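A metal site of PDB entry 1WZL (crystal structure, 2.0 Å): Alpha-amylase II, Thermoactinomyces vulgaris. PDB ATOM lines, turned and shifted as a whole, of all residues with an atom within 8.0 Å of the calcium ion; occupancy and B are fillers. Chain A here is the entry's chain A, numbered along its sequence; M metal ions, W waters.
Water W1 lies within hydrogen-bond range of the backbone carbonyl oxygen (O) of Gln 215 (2.6 Å) and the backbone carbonyl oxygen (O) of Asn 148 (3.4 Å).
OD2 of Asp 171 binds the calcium ion (2.3 Å).
OD2 of Asp 149 binds the calcium ion (2.3 Å).
OD1 of Asn 148 binds the calcium ion, at 2.4 Å.
O of Gly 169 binds the calcium ion (2.4 Å).
The calcium ion is bound by O of Asp 145 (2.5 Å).
The calcium ion is bound by the side-chain amide oxygen (OD1) of Asn 143 (2.5 Å).
Water W1 binds the calcium ion, 2.5 Å away.
The calcium ion has seven donor atoms within binding distance.
Six residues have an atom within 4 Å of the calcium ion: Asn 143, Asp 145, Asn 148, Asp 149, Gly 169 and Asp 171.
The nearest printed residue that does not touch the calcium ion is Pro 146 (4.2 Å).
The side-chain carboxylate (OD1) of Asp 171 is in hydrogen-bond range of the backbone NH (N) of Gly 144, at 2.9 Å.
N of Asp 171 is in hydrogen-bond range of O of Ala 142 (2.9 Å).
The backbone NH (N) of Lys 173 sits close to the side-chain carboxylate (OD1) of Asp 171, at 3.3 Å.
The side-chain carboxylate (OD1) of Asp 171 lies within hydrogen-bond range of the backbone NH (N) of Gly 174 (2.8 Å).
The backbone carbonyl oxygen (O) of Pro 138 is in hydrogen-bond range of the backbone NH (N) of Asp 171 (3.4 Å).
OE1 of Glu 139 lies within hydrogen-bond range of N of Gly 169, at 2.8 Å.
The side-chain hydroxyl (OG) of Ser 147 lies within hydrogen-bond range of the side-chain carboxylate (OD1) of Asp 145, at 2.5 Å.
The side-chain amide nitrogen of Asn 143 sits at hydrogen-bond distance from the backbone carbonyl oxygen of Tyr 168 (3.5 Å).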
ATOM      1  N   PRO A 138      15.351 -27.180  10.301  1.00  0.00           N
ATOM      2  CA  PRO A 138      15.670 -26.368  11.475  1.00  0.00           C
ATOM      3  C   PRO A 138      15.545 -26.972  12.881  1.00  0.00           C
ATOM      4  O   PRO A 138      16.464 -26.810  13.695  1.00  0.00           O
ATOM      5  CB  PRO A 138      14.808 -25.126  11.283  1.00  0.00           C
ATOM      6  CG  PRO A 138      13.689 -25.611  10.399  1.00  0.00           C
ATOM      7  CD  PRO A 138      14.391 -26.480   9.432  1.00  0.00           C
ATOM      8  N   GLU A 139      14.437 -27.662  13.156  1.00  0.00           N
ATOM      9  CA  GLU A 139      14.214 -28.267  14.475  1.00  0.00           C
ATOM     10  C   GLU A 139      15.333 -29.225  14.870  1.00  0.00           C
ATOM     11  O   GLU A 139      15.616 -29.407  16.062  1.00  0.00           O
ATOM     12  CB  GLU A 139      12.879 -29.035  14.490  1.00  0.00           C
ATOM     13  CG  GLU A 139      12.001 -28.808  15.724  1.00  0.00           C
ATOM     14  CD  GLU A 139      12.600 -29.334  17.020  1.00  0.00           C
ATOM     15  OE1 GLU A 139      12.848 -28.511  17.937  1.00  0.00           O
ATOM     16  OE2 GLU A 139      12.812 -30.561  17.140  1.00  0.00           O
ATOM     17  N   ALA A 142      20.668 -27.371  14.599  1.00  0.00           N
ATOM     18  CA  ALA A 142      21.494 -26.876  15.692  1.00  0.00           C
ATOM     19  C   ALA A 142      20.671 -25.998  16.618  1.00  0.00           C
ATOM     20  O   ALA A 142      19.966 -25.095  16.177  1.00  0.00           O
ATOM     21  CB  ALA A 142      22.687 -26.104  15.139  1.00  0.00           C
ATOM     22  N   ASN A 143      20.779 -26.258  17.917  1.00  0.00           N
ATOM     23  CA  ASN A 143      20.057 -25.489  18.939  1.00  0.00           C
ATOM     24  C   ASN A 143      21.015 -24.433  19.463  1.00  0.00           C
ATOM     25  O   ASN A 143      21.780 -24.685  20.398  1.00  0.00           O
ATOM     26  CB  ASN A 143      19.601 -26.406  20.075  1.00  0.00           C
ATOM     27  CG  ASN A 143      18.705 -25.709  21.086  1.00  0.00           C
ATOM     28  OD1 ASN A 143      18.483 -24.490  21.006  1.00  0.00           O
ATOM     29  ND2 ASN A 143      18.175 -26.469  22.041  1.00  0.00           N
ATOM     30  N   GLY A 144      21.000 -23.252  18.853  1.00  0.00           N
ATOM     31  CA  GLY A 144      21.884 -22.195  19.306  1.00  0.00           C
ATOM     32  C   GLY A 144      21.289 -21.349  20.405  1.00  0.00           C
ATOM     33  O   GLY A 144      22.012 -20.661  21.128  1.00  0.00           O
ATOM     34  N   ASP A 145      19.964 -21.412  20.544  1.00  0.00           N
ATOM     35  CA  ASP A 145      19.271 -20.642  21.551  1.00  0.00           C
ATOM     36  C   ASP A 145      18.348 -21.515  22.397  1.00  0.00           C
ATOM     37  O   ASP A 145      17.199 -21.742  22.030  1.00  0.00           O
ATOM     38  CB  ASP A 145      18.480 -19.523  20.872  1.00  0.00           C
ATOM     39  CG  ASP A 145      17.781 -18.608  21.860  1.00  0.00           C
ATOM     40  OD1 ASP A 145      17.925 -18.810  23.077  1.00  0.00           O
ATOM     41  OD2 ASP A 145      17.083 -17.682  21.392  1.00  0.00           O
ATOM     42  N   PRO A 146      18.842 -22.012  23.535  1.00  0.00           N
ATOM     43  CA  PRO A 146      18.062 -22.850  24.432  1.00  0.00           C
ATOM     44  C   PRO A 146      16.821 -22.134  24.975  1.00  0.00           C
ATOM     45  O   PRO A 146      15.807 -22.771  25.259  1.00  0.00           O
ATOM     46  CB  PRO A 146      19.039 -23.176  25.557  1.00  0.00           C
ATOM     47  CG  PRO A 146      20.372 -23.095  24.895  1.00  0.00           C
ATOM     48  CD  PRO A 146      20.235 -21.899  24.003  1.00  0.00           C
ATOM     49  N   SER A 147      16.911 -20.815  25.090  1.00  0.00           N
ATOM     50  CA  SER A 147      15.803 -20.024  25.652  1.00  0.00           C
ATOM     51  C   SER A 147      14.499 -20.064  24.869  1.00  0.00           C
ATOM     52  O   SER A 147      13.436 -19.751  25.416  1.00  0.00           O
ATOM     53  CB  SER A 147      16.223 -18.564  25.835  1.00  0.00           C
ATOM     54  OG  SER A 147      16.189 -17.849  24.608  1.00  0.00           O
ATOM     55  N   ASN A 148      14.549 -20.414  23.585  1.00  0.00           N
ATOM     56  CA  ASN A 148      13.311 -20.453  22.809  1.00  0.00           C
ATOM     57  C   ASN A 148      12.815 -21.882  22.580  1.00  0.00           C
ATOM     58  O   ASN A 148      11.949 -22.104  21.735  1.00  0.00           O
ATOM     59  CB  ASN A 148      13.489 -19.768  21.453  1.00  0.00           C
ATOM     60  CG  ASN A 148      14.537 -20.451  20.582  1.00  0.00           C
ATOM     61  OD1 ASN A 148      14.757 -21.655  20.675  1.00  0.00           O
ATOM     62  ND2 ASN A 148      15.183 -19.677  19.716  1.00  0.00           N
ATOM     63  N   ASP A 149      13.365 -22.828  23.325  1.00  0.00           N
ATOM     64  CA  ASP A 149      12.951 -24.226  23.161  1.00  0.00           C
ATOM     65  C   ASP A 149      11.493 -24.468  23.485  1.00  0.00           C
ATOM     66  O   ASP A 149      10.934 -23.891  24.410  1.00  0.00           O
ATOM     67  CB  ASP A 149      13.798 -25.156  24.028  1.00  0.00           C
ATOM     68  CG  ASP A 149      15.233 -25.262  23.538  1.00  0.00           C
ATOM     69  OD1 ASP A 149      16.025 -25.933  24.212  1.00  0.00           O
ATOM     70  OD2 ASP A 149      15.548 -24.660  22.485  1.00  0.00           O
ATOM     71  N   PRO A 150      10.836 -25.326  22.692  1.00  0.00           N
ATOM     72  CA  PRO A 150       9.434 -25.661  22.915  1.00  0.00           C
ATOM     73  C   PRO A 150       9.332 -26.498  24.181  1.00  0.00           C
ATOM     74  O   PRO A 150      10.306 -27.136  24.599  1.00  0.00           O
ATOM     75  CB  PRO A 150       9.065 -26.450  21.661  1.00  0.00           C
ATOM     76  CG  PRO A 150      10.005 -25.906  20.617  1.00  0.00           C
ATOM     77  CD  PRO A 150      11.301 -25.848  21.392  1.00  0.00           C
ATOM     78  N   THR A 153      11.163 -30.274  25.397  1.00  0.00           N
ATOM     79  CA  THR A 153      12.266 -30.577  24.482  1.00  0.00           C
ATOM     80  C   THR A 153      13.114 -31.729  25.052  1.00  0.00           C
ATOM     81  O   THR A 153      13.377 -31.767  26.257  1.00  0.00           O
ATOM     82  CB  THR A 153      13.185 -29.363  24.262  1.00  0.00           C
ATOM     83  OG1 THR A 153      12.426 -28.277  23.704  1.00  0.00           O
ATOM     84  CG2 THR A 153      14.327 -29.714  23.316  1.00  0.00           C
ATOM     85  N   TRP A 156      19.749 -33.676  23.332  1.00  0.00           N
ATOM     86  CA  TRP A 156      20.365 -33.755  22.017  1.00  0.00           C
ATOM     87  C   TRP A 156      21.479 -34.792  22.051  1.00  0.00           C
ATOM     88  O   TRP A 156      22.613 -34.479  22.423  1.00  0.00           O
ATOM     89  CB  TRP A 156      20.937 -32.389  21.639  1.00  0.00           C
ATOM     90  CG  TRP A 156      21.272 -32.226  20.191  1.00  0.00           C
ATOM     91  CD1 TRP A 156      22.296 -32.814  19.502  1.00  0.00           C
ATOM     92  CD2 TRP A 156      20.577 -31.393  19.253  1.00  0.00           C
ATOM     93  NE1 TRP A 156      22.288 -32.395  18.194  1.00  0.00           N
ATOM     94  CE2 TRP A 156      21.240 -31.526  18.008  1.00  0.00           C
ATOM     95  CE3 TRP A 156      19.458 -30.550  19.342  1.00  0.00           C
ATOM     96  CZ2 TRP A 156      20.824 -30.841  16.855  1.00  0.00           C
ATOM     97  CZ3 TRP A 156      19.046 -29.871  18.196  1.00  0.00           C
ATOM     98  CH2 TRP A 156      19.720 -30.021  16.973  1.00  0.00           C
ATOM     99  N   TYR A 168      13.690 -31.016  19.745  1.00  0.00           N
ATOM    100  CA  TYR A 168      15.090 -30.980  20.149  1.00  0.00           C
ATOM    101  C   TYR A 168      15.624 -29.553  20.275  1.00  0.00           C
ATOM    102  O   TYR A 168      16.755 -29.341  20.721  1.00  0.00           O
ATOM    103  CB  TYR A 168      15.943 -31.764  19.160  1.00  0.00           C
ATOM    104  CG  TYR A 168      15.713 -33.255  19.254  1.00  0.00           C
ATOM    105  CD1 TYR A 168      16.316 -34.017  20.253  1.00  0.00           C
ATOM    106  CD2 TYR A 168      14.836 -33.892  18.374  1.00  0.00           C
ATOM    107  CE1 TYR A 168      16.055 -35.374  20.386  1.00  0.00           C
ATOM    108  CE2 TYR A 168      14.562 -35.254  18.496  1.00  0.00           C
ATOM    109  CZ  TYR A 168      15.169 -35.984  19.504  1.00  0.00           C
ATOM    110  OH  TYR A 168      14.900 -37.330  19.623  1.00  0.00           O
ATOM    111  N   GLY A 169      14.799 -28.580  19.909  1.00  0.00           N
ATOM    112  CA  GLY A 169      15.194 -27.183  20.041  1.00  0.00           C
ATOM    113  C   GLY A 169      15.997 -26.539  18.926  1.00  0.00           C
ATOM    114  O   GLY A 169      16.520 -25.440  19.115  1.00  0.00           O
ATOM    115  N   GLY A 170      16.095 -27.207  17.778  1.00  0.00           N
ATOM    116  CA  GLY A 170      16.848 -26.639  16.670  1.00  0.00           C
ATOM    117  C   GLY A 170      16.299 -25.271  16.297  1.00  0.00           C
ATOM    118  O   GLY A 170      15.084 -25.066  16.344  1.00  0.00           O
ATOM    119  N   ASP A 171      17.178 -24.333  15.935  1.00  0.00           N
ATOM    120  CA  ASP A 171      16.723 -22.984  15.609  1.00  0.00           C
ATOM    121  C   ASP A 171      17.627 -22.215  14.651  1.00  0.00           C
ATOM    122  O   ASP A 171      18.674 -22.716  14.237  1.00  0.00           O
ATOM    123  CB  ASP A 171      16.542 -22.191  16.910  1.00  0.00           C
ATOM    124  CG  ASP A 171      17.754 -22.257  17.794  1.00  0.00           C
ATOM    125  OD1 ASP A 171      18.879 -22.160  17.263  1.00  0.00           O
ATOM    126  OD2 ASP A 171      17.569 -22.394  19.023  1.00  0.00           O
ATOM    127  N   LEU A 172      17.223 -20.984  14.302  1.00  0.00           N
ATOM    128  CA  LEU A 172      18.001 -20.156  13.385  1.00  0.00           C
ATOM    129  C   LEU A 172      19.335 -19.724  13.997  1.00  0.00           C
ATOM    130  O   LEU A 172      20.328 -19.580  13.269  1.00  0.00           O
ATOM    131  CB  LEU A 172      17.210 -18.923  12.960  1.00  0.00           C
ATOM    132  CG  LEU A 172      15.887 -19.211  12.224  1.00  0.00           C
ATOM    133  CD1 LEU A 172      15.277 -17.915  11.743  1.00  0.00           C
ATOM    134  CD2 LEU A 172      16.133 -20.162  11.026  1.00  0.00           C
ATOM    135  N   LYS A 173      19.362 -19.504  15.304  1.00  0.00           N
ATOM    136  CA  LYS A 173      20.613 -19.110  15.968  1.00  0.00           C
ATOM    137  C   LYS A 173      21.633 -20.230  15.793  1.00  0.00           C
ATOM    138  O   LYS A 173      22.826 -19.974  15.627  1.00  0.00           O
ATOM    139  CB  LYS A 173      20.382 -18.864  17.467  1.00  0.00           C
ATOM    140  CG  LYS A 173      21.652 -18.407  18.198  1.00  0.00           C
ATOM    141  CD  LYS A 173      21.992 -16.958  17.852  1.00  0.00           C
ATOM    142  CE  LYS A 173      23.487 -16.671  17.886  1.00  0.00           C
ATOM    143  NZ  LYS A 173      24.181 -17.240  19.086  1.00  0.00           N
ATOM    144  N   GLY A 174      21.164 -21.474  15.846  1.00  0.00           N
ATOM    145  CA  GLY A 174      22.058 -22.604  15.672  1.00  0.00           C
ATOM    146  C   GLY A 174      22.673 -22.591  14.293  1.00  0.00           C
ATOM    147  O   GLY A 174      23.874 -22.787  14.123  1.00  0.00           O
ATOM    148  N   PRO A 214       8.220 -18.539  16.660  1.00  0.00           N
ATOM    149  CA  PRO A 214       8.926 -18.230  17.901  1.00  0.00           C
ATOM    150  C   PRO A 214       9.960 -19.264  18.333  1.00  0.00           C
ATOM    151  O   PRO A 214      10.992 -18.904  18.903  1.00  0.00           O
ATOM    152  CB  PRO A 214       7.790 -18.088  18.912  1.00  0.00           C
ATOM    153  CG  PRO A 214       6.689 -17.514  18.057  1.00  0.00           C
ATOM    154  CD  PRO A 214       6.773 -18.357  16.820  1.00  0.00           C
ATOM    155  N   GLN A 215       9.711 -20.541  18.072  1.00  0.00           N
ATOM    156  CA  GLN A 215      10.679 -21.554  18.485  1.00  0.00           C
ATOM    157  C   GLN A 215      11.952 -21.551  17.629  1.00  0.00           C
ATOM    158  O   GLN A 215      12.992 -22.048  18.056  1.00  0.00           O
ATOM    159  CB  GLN A 215      10.047 -22.952  18.472  1.00  0.00           C
ATOM    160  CG  GLN A 215       9.836 -23.550  17.097  1.00  0.00           C
ATOM    161  CD  GLN A 215       9.204 -24.920  17.160  1.00  0.00           C
ATOM    162  OE1 GLN A 215       7.979 -25.061  17.215  1.00  0.00           O
ATOM    163  NE2 GLN A 215      10.045 -25.957  17.181  1.00  0.00           N
ATOM    164  N   PHE A 216      11.869 -20.970  16.431  1.00  0.00           N
ATOM    165  CA  PHE A 216      13.033 -20.915  15.547  1.00  0.00           C
ATOM    166  C   PHE A 216      13.793 -19.595  15.668  1.00  0.00           C
ATOM    167  O   PHE A 216      15.005 -19.554  15.528  1.00  0.00           O
ATOM    168  CB  PHE A 216      12.613 -21.118  14.082  1.00  0.00           C
ATOM    169  CG  PHE A 216      12.107 -22.503  13.783  1.00  0.00           C
ATOM    170  CD1 PHE A 216      12.671 -23.618  14.388  1.00  0.00           C
ATOM    171  CD2 PHE A 216      11.078 -22.678  12.864  1.00  0.00           C
ATOM    172  CE1 PHE A 216      12.217 -24.906  14.071  1.00  0.00           C
ATOM    173  CE2 PHE A 216      10.619 -23.953  12.547  1.00  0.00           C
ATOM    174  CZ  PHE A 216      11.183 -25.068  13.151  1.00  0.00           C
ATOM    175  N   GLY A 217      13.057 -18.519  15.926  1.00  0.00           N
ATOM    176  CA  GLY A 217      13.679 -17.219  16.073  1.00  0.00           C
ATOM    177  C   GLY A 217      12.711 -16.073  15.859  1.00  0.00           C
ATOM    178  O   GLY A 217      11.537 -16.152  16.223  1.00  0.00           O
HETATM  179 CA    CA M   1      16.222 -23.504  20.565  1.00  0.00          CA
HETATM  180  O   HOH W   1      13.932 -23.957  19.611  1.00  0.00           O
